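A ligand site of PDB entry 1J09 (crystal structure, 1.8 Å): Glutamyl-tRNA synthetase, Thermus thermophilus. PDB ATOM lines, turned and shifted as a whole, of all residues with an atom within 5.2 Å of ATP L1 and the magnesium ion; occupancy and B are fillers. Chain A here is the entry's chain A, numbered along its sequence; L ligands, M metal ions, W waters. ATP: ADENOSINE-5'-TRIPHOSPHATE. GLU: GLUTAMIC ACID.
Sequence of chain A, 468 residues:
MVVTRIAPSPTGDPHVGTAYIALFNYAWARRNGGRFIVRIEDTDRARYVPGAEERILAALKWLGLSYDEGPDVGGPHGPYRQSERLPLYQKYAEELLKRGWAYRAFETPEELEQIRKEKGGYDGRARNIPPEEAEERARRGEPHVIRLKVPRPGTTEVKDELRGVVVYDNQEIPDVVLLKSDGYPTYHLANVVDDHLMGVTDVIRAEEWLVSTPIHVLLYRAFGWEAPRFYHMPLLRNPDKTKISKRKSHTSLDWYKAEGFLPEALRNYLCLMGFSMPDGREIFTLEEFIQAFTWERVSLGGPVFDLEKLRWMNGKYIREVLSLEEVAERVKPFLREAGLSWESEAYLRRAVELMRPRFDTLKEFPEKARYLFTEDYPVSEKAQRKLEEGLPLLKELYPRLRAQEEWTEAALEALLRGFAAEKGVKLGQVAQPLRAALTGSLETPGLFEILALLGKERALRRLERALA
O of Ile 244 sits at hydrogen-bond distance from N6 of ATP L1, 3.0 Å away. An oxygen (O2B) of ATP L1 sits at hydrogen-bond distance from a ring nitrogen (NE2) of His 15, at 2.9 Å. The backbone NH (N) of Lys 246 lies within hydrogen-bond range of an oxygen (O2B) of ATP L1 (2.8 Å). The backbone NH of Leu 236 sits at hydrogen-bond distance from a nitrogen (N1) of ATP L1 (2.9 Å). The side-chain amino group (NZ) of Lys 246 is in salt-bridge range of an oxygen (O2A) of ATP L1. NZ of Lys 243 is in salt-bridge range of O2B of ATP L1 (3.7 Å). O of Leu 236 is in hydrogen-bond range of N6 of ATP L1 (3.0 Å). The guanidinium group (NE) of Arg 247 lies within salt-bridge range of an oxygen (O3G) of ATP L1. An oxygen (O2') of ATP L1 sits at hydrogen-bond distance from the side-chain carboxylate (OE2) of Glu 208 (2.7 Å). An oxygen (O2') of ATP L1 sits at hydrogen-bond distance from the indole nitrogen of Trp 209 (3.0 Å). The side-chain hydroxyl of Ser 245 is in hydrogen-bond range of an oxygen (O2G) of ATP L1, 2.7 Å away.
An oxygen (O3') of ATP L1 sits at hydrogen-bond distance from an oxygen (OXT) of GLU L2, at 2.7 Å.
O of Pro 234 is in hydrogen-bond range of OH of Tyr 20, at 2.8 Å. OG of Ser 245 sits close to N of Arg 247, at 3.1 Å. NZ of Lys 246 lies within hydrogen-bond range of OG1 of Thr 11 (3.4 Å). The backbone carbonyl oxygen of Leu 236 is in hydrogen-bond range of the backbone NH of Ile 244 (2.9 Å). N of Gly 17 is in hydrogen-bond range of ND1 of His 15, at 2.8 Å. The backbone carbonyl oxygen of Leu 235 is in hydrogen-bond range of the guanidinium group of Arg 237 (3.0 Å).
Residues that only touch ATP L1: Leu 235 (3.5 Å), Gly 17 (3.7 Å), Ala 206 (3.9 Å), Thr 18 (3.98 Å) and Tyr 20 (3.99 Å). Within 4 Å of ATP L1: His 15, Gly 17, Thr 18, Tyr 20, Ala 206, Glu 208, Trp 209, Leu 235, Leu 236, Lys 243, Ile 244, Ser 245, Lys 246 and Arg 247. The nearest printed residue that does not touch ATP L1 is Thr 11 (4.3 Å).
No residue comes within 4 Å of the magnesium ion. The nearest printed residue that does not touch the magnesium ion is Glu 208 (4.2 Å).
Water W12 binds the magnesium ion (2.0 Å). The magnesium ion is bound by water W3 (2.0 Å). Water W8 is bound to the magnesium ion (2.0 Å). O1A of ATP L1 is bound to the magnesium ion, at 2.0 Å. O1B of ATP L1 binds the magnesium ion (2.1 Å). O1G of ATP L1 is bound to the magnesium ion (2.1 Å).
Water W3 lies within hydrogen-bond range of the side-chain carboxylate of Glu 208 (2.6 Å) and an oxygen (O5') of ATP L1 (3.2 Å). Water W4 lies within hydrogen-bond range of O2G of ATP L1 and NZ of Lys 243. Water W11 bridges an oxygen (O3') of ATP L1 (2.7 Å) and the backbone carbonyl oxygen (O) of Gly 17 (3.1 Å). Water W13 lies within hydrogen-bond range of the side-chain hydroxyl of Thr 18 (2.7 Å) and an oxygen (O3') of ATP L1 (2.8 Å). Water W10 lies within hydrogen-bond range of N of Ala 206 (2.9 Å), NE1 of Trp 209 (3.3 Å) and O2' of ATP L1 (3.3 Å). Water W2 bridges an oxygen (O) of GLU L2 (2.8 Å) and an oxygen (O5') of ATP L1 (3.3 Å).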
ATOM      1  N   THR A  11     -17.954   1.962  -0.395  1.00  0.00           N
ATOM      2  CA  THR A  11     -17.936   2.096  -1.844  1.00  0.00           C
ATOM      3  C   THR A  11     -19.361   2.205  -2.357  1.00  0.00           C
ATOM      4  O   THR A  11     -19.682   3.090  -3.139  1.00  0.00           O
ATOM      5  CB  THR A  11     -17.258   0.893  -2.534  1.00  0.00           C
ATOM      6  OG1 THR A  11     -17.973  -0.310  -2.209  1.00  0.00           O
ATOM      7  CG2 THR A  11     -15.822   0.756  -2.071  1.00  0.00           C
ATOM      8  N   HIS A  15     -20.713  -4.372   2.843  1.00  0.00           N
ATOM      9  CA  HIS A  15     -20.208  -5.698   2.465  1.00  0.00           C
ATOM     10  C   HIS A  15     -20.303  -6.743   3.592  1.00  0.00           C
ATOM     11  O   HIS A  15     -19.993  -6.458   4.746  1.00  0.00           O
ATOM     12  CB  HIS A  15     -18.753  -5.538   2.001  1.00  0.00           C
ATOM     13  CG  HIS A  15     -18.266  -6.635   1.109  1.00  0.00           C
ATOM     14  ND1 HIS A  15     -18.114  -7.940   1.542  1.00  0.00           N
ATOM     15  CD2 HIS A  15     -17.832  -6.608  -0.171  1.00  0.00           C
ATOM     16  CE1 HIS A  15     -17.612  -8.669   0.566  1.00  0.00           C
ATOM     17  NE2 HIS A  15     -17.427  -7.885  -0.488  1.00  0.00           N
ATOM     18  N   GLY A  17     -18.416  -9.004   4.071  1.00  0.00           N
ATOM     19  CA  GLY A  17     -17.056  -9.175   4.555  1.00  0.00           C
ATOM     20  C   GLY A  17     -16.780  -8.233   5.714  1.00  0.00           C
ATOM     21  O   GLY A  17     -16.012  -8.542   6.620  1.00  0.00           O
ATOM     22  N   THR A  18     -17.389  -7.054   5.685  1.00  0.00           N
ATOM     23  CA  THR A  18     -17.216  -6.072   6.751  1.00  0.00           C
ATOM     24  C   THR A  18     -17.885  -6.589   8.028  1.00  0.00           C
ATOM     25  O   THR A  18     -17.362  -6.425   9.127  1.00  0.00           O
ATOM     26  CB  THR A  18     -17.841  -4.708   6.362  1.00  0.00           C
ATOM     27  OG1 THR A  18     -17.202  -4.205   5.178  1.00  0.00           O
ATOM     28  CG2 THR A  18     -17.686  -3.690   7.488  1.00  0.00           C
ATOM     29  N   TYR A  20     -18.461  -9.803   8.801  1.00  0.00           N
ATOM     30  CA  TYR A  20     -17.680 -10.961   9.239  1.00  0.00           C
ATOM     31  C   TYR A  20     -16.488 -10.514  10.079  1.00  0.00           C
ATOM     32  O   TYR A  20     -16.284 -10.996  11.189  1.00  0.00           O
ATOM     33  CB  TYR A  20     -17.222 -11.738   7.994  1.00  0.00           C
ATOM     34  CG  TYR A  20     -16.080 -12.723   8.183  1.00  0.00           C
ATOM     35  CD1 TYR A  20     -16.174 -13.793   9.070  1.00  0.00           C
ATOM     36  CD2 TYR A  20     -14.932 -12.624   7.390  1.00  0.00           C
ATOM     37  CE1 TYR A  20     -15.138 -14.752   9.164  1.00  0.00           C
ATOM     38  CE2 TYR A  20     -13.906 -13.565   7.473  1.00  0.00           C
ATOM     39  CZ  TYR A  20     -14.009 -14.625   8.358  1.00  0.00           C
ATOM     40  OH  TYR A  20     -12.992 -15.553   8.394  1.00  0.00           O
ATOM     41  N   ILE A  21     -15.704  -9.588   9.536  1.00  0.00           N
ATOM     42  CA  ILE A  21     -14.532  -9.075  10.251  1.00  0.00           C
ATOM     43  C   ILE A  21     -14.949  -8.300  11.493  1.00  0.00           C
ATOM     44  O   ILE A  21     -14.309  -8.416  12.546  1.00  0.00           O
ATOM     45  CB  ILE A  21     -13.685  -8.163   9.338  1.00  0.00           C
ATOM     46  CG1 ILE A  21     -13.140  -8.974   8.163  1.00  0.00           C
ATOM     47  CG2 ILE A  21     -12.558  -7.514  10.127  1.00  0.00           C
ATOM     48  CD1 ILE A  21     -12.282 -10.171   8.568  1.00  0.00           C
ATOM     49  N   ALA A 206      -9.114  -9.296   7.214  1.00  0.00           N
ATOM     50  CA  ALA A 206      -9.088 -10.391   6.230  1.00  0.00           C
ATOM     51  C   ALA A 206      -7.663 -10.699   5.760  1.00  0.00           C
ATOM     52  O   ALA A 206      -6.831  -9.795   5.636  1.00  0.00           O
ATOM     53  CB  ALA A 206      -9.974 -10.023   5.046  1.00  0.00           C
ATOM     54  N   GLU A 208      -6.370 -11.127   3.011  1.00  0.00           N
ATOM     55  CA  GLU A 208      -5.878 -10.457   1.814  1.00  0.00           C
ATOM     56  C   GLU A 208      -4.987  -9.271   2.171  1.00  0.00           C
ATOM     57  O   GLU A 208      -4.259  -8.744   1.321  1.00  0.00           O
ATOM     58  CB  GLU A 208      -7.040 -10.008   0.908  1.00  0.00           C
ATOM     59  CG  GLU A 208      -7.946  -8.915   1.477  1.00  0.00           C
ATOM     60  CD  GLU A 208      -8.996  -8.471   0.484  1.00  0.00           C
ATOM     61  OE1 GLU A 208      -8.906  -8.888  -0.692  1.00  0.00           O
ATOM     62  OE2 GLU A 208      -9.915  -7.725   0.861  1.00  0.00           O
ATOM     63  N   TRP A 209      -5.031  -8.850   3.432  1.00  0.00           N
ATOM     64  CA  TRP A 209      -4.202  -7.730   3.883  1.00  0.00           C
ATOM     65  C   TRP A 209      -2.887  -8.213   4.489  1.00  0.00           C
ATOM     66  O   TRP A 209      -2.005  -7.414   4.779  1.00  0.00           O
ATOM     67  CB  TRP A 209      -4.970  -6.890   4.920  1.00  0.00           C
ATOM     68  CG  TRP A 209      -6.264  -6.324   4.401  1.00  0.00           C
ATOM     69  CD1 TRP A 209      -7.523  -6.804   4.639  1.00  0.00           C
ATOM     70  CD2 TRP A 209      -6.411  -5.224   3.504  1.00  0.00           C
ATOM     71  NE1 TRP A 209      -8.445  -6.058   3.943  1.00  0.00           N
ATOM     72  CE2 TRP A 209      -7.790  -5.080   3.241  1.00  0.00           C
ATOM     73  CE3 TRP A 209      -5.511  -4.328   2.906  1.00  0.00           C
ATOM     74  CZ2 TRP A 209      -8.297  -4.087   2.389  1.00  0.00           C
ATOM     75  CZ3 TRP A 209      -6.018  -3.342   2.060  1.00  0.00           C
ATOM     76  CH2 TRP A 209      -7.397  -3.222   1.816  1.00  0.00           C
ATOM     77  N   PRO A 234      -9.373 -15.885   7.707  1.00  0.00           N
ATOM     78  CA  PRO A 234      -9.456 -16.494   6.370  1.00  0.00           C
ATOM     79  C   PRO A 234     -10.506 -15.752   5.558  1.00  0.00           C
ATOM     80  O   PRO A 234     -11.501 -15.262   6.094  1.00  0.00           O
ATOM     81  CB  PRO A 234      -9.911 -17.926   6.664  1.00  0.00           C
ATOM     82  CG  PRO A 234      -9.475 -18.174   8.080  1.00  0.00           C
ATOM     83  CD  PRO A 234      -9.760 -16.845   8.749  1.00  0.00           C
ATOM     84  N   LEU A 235     -10.281 -15.672   4.249  1.00  0.00           N
ATOM     85  CA  LEU A 235     -11.247 -15.011   3.383  1.00  0.00           C
ATOM     86  C   LEU A 235     -12.449 -15.926   3.222  1.00  0.00           C
ATOM     87  O   LEU A 235     -12.308 -17.151   3.243  1.00  0.00           O
ATOM     88  CB  LEU A 235     -10.652 -14.745   2.000  1.00  0.00           C
ATOM     89  CG  LEU A 235      -9.643 -13.599   1.859  1.00  0.00           C
ATOM     90  CD1 LEU A 235      -8.851 -13.768   0.573  1.00  0.00           C
ATOM     91  CD2 LEU A 235     -10.380 -12.276   1.867  1.00  0.00           C
ATOM     92  N   LEU A 236     -13.625 -15.345   3.073  1.00  0.00           N
ATOM     93  CA  LEU A 236     -14.841 -16.121   2.862  1.00  0.00           C
ATOM     94  C   LEU A 236     -14.725 -16.617   1.425  1.00  0.00           C
ATOM     95  O   LEU A 236     -14.350 -15.856   0.534  1.00  0.00           O
ATOM     96  CB  LEU A 236     -16.073 -15.215   3.022  1.00  0.00           C
ATOM     97  CG  LEU A 236     -16.258 -14.581   4.407  1.00  0.00           C
ATOM     98  CD1 LEU A 236     -17.445 -13.656   4.369  1.00  0.00           C
ATOM     99  CD2 LEU A 236     -16.456 -15.661   5.459  1.00  0.00           C
ATOM    100  N   ARG A 237     -15.045 -17.887   1.201  1.00  0.00           N
ATOM    101  CA  ARG A 237     -14.919 -18.475  -0.126  1.00  0.00           C
ATOM    102  C   ARG A 237     -16.206 -18.988  -0.761  1.00  0.00           C
ATOM    103  O   ARG A 237     -17.169 -19.306  -0.081  1.00  0.00           O
ATOM    104  CB  ARG A 237     -13.924 -19.645  -0.088  1.00  0.00           C
ATOM    105  CG  ARG A 237     -12.677 -19.423   0.744  1.00  0.00           C
ATOM    106  CD  ARG A 237     -11.830 -18.279   0.216  1.00  0.00           C
ATOM    107  NE  ARG A 237     -10.604 -18.127   0.992  1.00  0.00           N
ATOM    108  CZ  ARG A 237      -9.551 -18.931   0.912  1.00  0.00           C
ATOM    109  NH1 ARG A 237      -9.566 -19.962   0.072  1.00  0.00           N
ATOM    110  NH2 ARG A 237      -8.486 -18.709   1.664  1.00  0.00           N
ATOM    111  N   LYS A 243     -12.230 -16.735  -3.726  1.00  0.00           N
ATOM    112  CA  LYS A 243     -12.618 -15.672  -2.796  1.00  0.00           C
ATOM    113  C   LYS A 243     -13.965 -15.034  -3.144  1.00  0.00           C
ATOM    114  O   LYS A 243     -14.235 -14.709  -4.289  1.00  0.00           O
ATOM    115  CB  LYS A 243     -11.548 -14.590  -2.778  1.00  0.00           C
ATOM    116  CG  LYS A 243     -11.996 -13.258  -2.200  1.00  0.00           C
ATOM    117  CD  LYS A 243     -10.994 -12.154  -2.522  1.00  0.00           C
ATOM    118  CE  LYS A 243     -11.498 -10.809  -2.039  1.00  0.00           C
ATOM    119  NZ  LYS A 243     -12.795 -10.431  -2.649  1.00  0.00           N
ATOM    120  N   ILE A 244     -14.826 -14.862  -2.142  1.00  0.00           N
ATOM    121  CA  ILE A 244     -16.114 -14.231  -2.388  1.00  0.00           C
ATOM    122  C   ILE A 244     -15.851 -12.787  -2.810  1.00  0.00           C
ATOM    123  O   ILE A 244     -15.003 -12.127  -2.229  1.00  0.00           O
ATOM    124  CB  ILE A 244     -17.001 -14.264  -1.128  1.00  0.00           C
ATOM    125  CG1 ILE A 244     -17.597 -15.671  -0.979  1.00  0.00           C
ATOM    126  CG2 ILE A 244     -18.108 -13.208  -1.213  1.00  0.00           C
ATOM    127  CD1 ILE A 244     -18.525 -15.817   0.186  1.00  0.00           C
ATOM    128  N   SER A 245     -16.581 -12.326  -3.813  1.00  0.00           N
ATOM    129  CA  SER A 245     -16.428 -10.971  -4.331  1.00  0.00           C
ATOM    130  C   SER A 245     -17.766 -10.327  -4.688  1.00  0.00           C
ATOM    131  O   SER A 245     -18.664 -10.986  -5.219  1.00  0.00           O
ATOM    132  CB  SER A 245     -15.526 -10.988  -5.572  1.00  0.00           C
ATOM    133  OG  SER A 245     -15.660  -9.787  -6.311  1.00  0.00           O
ATOM    134  N   LYS A 246     -17.881  -9.029  -4.411  1.00  0.00           N
ATOM    135  CA  LYS A 246     -19.099  -8.274  -4.694  1.00  0.00           C
ATOM    136  C   LYS A 246     -19.387  -8.208  -6.194  1.00  0.00           C
ATOM    137  O   LYS A 246     -20.498  -7.906  -6.611  1.00  0.00           O
ATOM    138  CB  LYS A 246     -18.972  -6.846  -4.143  1.00  0.00           C
ATOM    139  CG  LYS A 246     -17.919  -5.994  -4.843  1.00  0.00           C
ATOM    140  CD  LYS A 246     -17.741  -4.642  -4.131  1.00  0.00           C
ATOM    141  CE  LYS A 246     -16.688  -3.789  -4.832  1.00  0.00           C
ATOM    142  NZ  LYS A 246     -16.318  -2.578  -4.041  1.00  0.00           N
ATOM    143  N   ARG A 247     -18.379  -8.482  -7.005  1.00  0.00           N
ATOM    144  CA  ARG A 247     -18.533  -8.453  -8.455  1.00  0.00           C
ATOM    145  C   ARG A 247     -19.030  -9.793  -8.990  1.00  0.00           C
ATOM    146  O   ARG A 247     -19.411  -9.890 -10.166  1.00  0.00           O
ATOM    147  CB  ARG A 247     -17.206  -8.093  -9.116  1.00  0.00           C
ATOM    148  CG  ARG A 247     -16.628  -6.758  -8.668  1.00  0.00           C
ATOM    149  CD  ARG A 247     -15.248  -6.526  -9.265  1.00  0.00           C
ATOM    150  NE  ARG A 247     -14.664  -5.258  -8.820  1.00  0.00           N
ATOM    151  CZ  ARG A 247     -15.121  -4.068  -9.187  1.00  0.00           C
ATOM    152  NH1 ARG A 247     -16.165  -3.969 -10.002  1.00  0.00           N
ATOM    153  NH2 ARG A 247     -14.533  -2.968  -8.744  1.00  0.00           N
ATOM    154  N   THR A 251     -23.072  -9.881  -1.882  1.00  0.00           N
ATOM    155  CA  THR A 251     -22.296  -9.602  -0.689  1.00  0.00           C
ATOM    156  C   THR A 251     -22.916  -8.457   0.103  1.00  0.00           C
ATOM    157  O   THR A 251     -22.496  -8.152   1.218  1.00  0.00           O
ATOM    158  CB  THR A 251     -20.852  -9.201  -1.043  1.00  0.00           C
ATOM    159  OG1 THR A 251     -20.889  -8.124  -1.986  1.00  0.00           O
ATOM    160  CG2 THR A 251     -20.106 -10.383  -1.659  1.00  0.00           C
HETATM  161  PG  ATP L   1     -13.466  -6.729  -5.383  1.00  0.00           P
HETATM  162  O1G ATP L   1     -12.148  -6.545  -4.647  1.00  0.00           O
HETATM  163  O2G ATP L   1     -13.515  -8.113  -5.991  1.00  0.00           O
HETATM  164  O3G ATP L   1     -13.582  -5.680  -6.471  1.00  0.00           O
HETATM  165  PB  ATP L   1     -14.686  -7.164  -2.832  1.00  0.00           P
HETATM  166  O1B ATP L   1     -13.300  -7.487  -2.442  1.00  0.00           O
HETATM  167  O2B ATP L   1     -15.742  -8.210  -2.790  1.00  0.00           O
HETATM  168  O3B ATP L   1     -14.709  -6.548  -4.350  1.00  0.00           O
HETATM  169  PA  ATP L   1     -14.258  -4.715  -1.440  1.00  0.00           P
HETATM  170  O1A ATP L   1     -12.985  -4.825  -2.191  1.00  0.00           O
HETATM  171  O2A ATP L   1     -15.076  -3.473  -1.548  1.00  0.00           O
HETATM  172  O3A ATP L   1     -15.230  -5.939  -1.907  1.00  0.00           O
HETATM  173  O5' ATP L   1     -13.969  -5.018   0.100  1.00  0.00           O
HETATM  174  C5' ATP L   1     -14.884  -4.623   1.111  1.00  0.00           C
HETATM  175  C4' ATP L   1     -14.455  -5.163   2.465  1.00  0.00           C
HETATM  176  O4' ATP L   1     -14.769  -6.582   2.535  1.00  0.00           O
HETATM  177  C3' ATP L   1     -12.972  -5.052   2.789  1.00  0.00           C
HETATM  178  O3' ATP L   1     -12.800  -4.849   4.194  1.00  0.00           O
HETATM  179  C2' ATP L   1     -12.436  -6.410   2.355  1.00  0.00           C
HETATM  180  O2' ATP L   1     -11.230  -6.804   2.993  1.00  0.00           O
HETATM  181  C1' ATP L   1     -13.589  -7.329   2.748  1.00  0.00           C
HETATM  182  N9  ATP L   1     -13.678  -8.542   1.938  1.00  0.00           N
HETATM  183  C8  ATP L   1     -13.782  -8.634   0.576  1.00  0.00           C
HETATM  184  N7  ATP L   1     -13.881  -9.865   0.126  1.00  0.00           N
HETATM  185  C5  ATP L   1     -13.834 -10.633   1.279  1.00  0.00           C
HETATM  186  C6  ATP L   1     -13.891 -12.030   1.487  1.00  0.00           C
HETATM  187  N6  ATP L   1     -14.012 -12.921   0.502  1.00  0.00           N
HETATM  188  N1  ATP L   1     -13.814 -12.480   2.765  1.00  0.00           N
HETATM  189  C2  ATP L   1     -13.681 -11.576   3.748  1.00  0.00           C
HETATM  190  N3  ATP L   1     -13.609 -10.246   3.681  1.00  0.00           N
HETATM  191  C4  ATP L   1     -13.696  -9.837   2.400  1.00  0.00           C
HETATM  192  N   GLU L   2     -10.011   0.089   4.635  1.00  0.00           N
HETATM  193  CA  GLU L   2      -9.390  -1.230   4.554  1.00  0.00           C
HETATM  194  C   GLU L   2     -10.424  -2.253   4.049  1.00  0.00           C
HETATM  195  O   GLU L   2     -11.173  -1.881   3.125  1.00  0.00           O
HETATM  196  CB  GLU L   2      -8.848  -1.625   5.930  1.00  0.00           C
HETATM  197  CG  GLU L   2      -7.972  -2.867   5.942  1.00  0.00           C
HETATM  198  CD  GLU L   2      -7.381  -3.135   7.317  1.00  0.00           C
HETATM  199  OE1 GLU L   2      -6.249  -2.679   7.593  1.00  0.00           O
HETATM  200  OE2 GLU L   2      -8.064  -3.794   8.129  1.00  0.00           O
HETATM  201  OXT GLU L   2     -10.659  -3.280   4.736  1.00  0.00           O
HETATM  202 MG    MG M   1     -11.647  -6.273  -2.645  1.00  0.00          MG
HETATM  203  O   HOH W   1     -12.368  -8.252  -8.538  1.00  0.00           O
HETATM  204  O   HOH W   2     -11.229  -3.159   0.585  1.00  0.00           O
HETATM  205  O   HOH W   3     -11.002  -5.979  -0.793  1.00  0.00           O
HETATM  206  O   HOH W   4     -12.034 -10.118  -5.302  1.00  0.00           O
HETATM  207  O   HOH W   5     -13.865  -1.861   3.083  1.00  0.00           O
HETATM  208  O   HOH W   6      -9.865  -6.179  -6.184  1.00  0.00           O
HETATM  209  O   HOH W   7     -13.672  -1.345  -0.017  1.00  0.00           O
HETATM  210  O   HOH W   8     -10.399  -7.812  -2.781  1.00  0.00           O
HETATM  211  O   HOH W   9     -17.165  -2.312  -0.440  1.00  0.00           O
HETATM  212  O   HOH W  10     -10.604  -7.019   6.241  1.00  0.00           O
HETATM  213  O   HOH W  11     -13.675  -6.600   6.011  1.00  0.00           O
HETATM  214  O   HOH W  12     -10.306  -4.950  -3.256  1.00  0.00           O
HETATM  215  O   HOH W  13     -14.661  -3.524   5.761  1.00  0.00           O
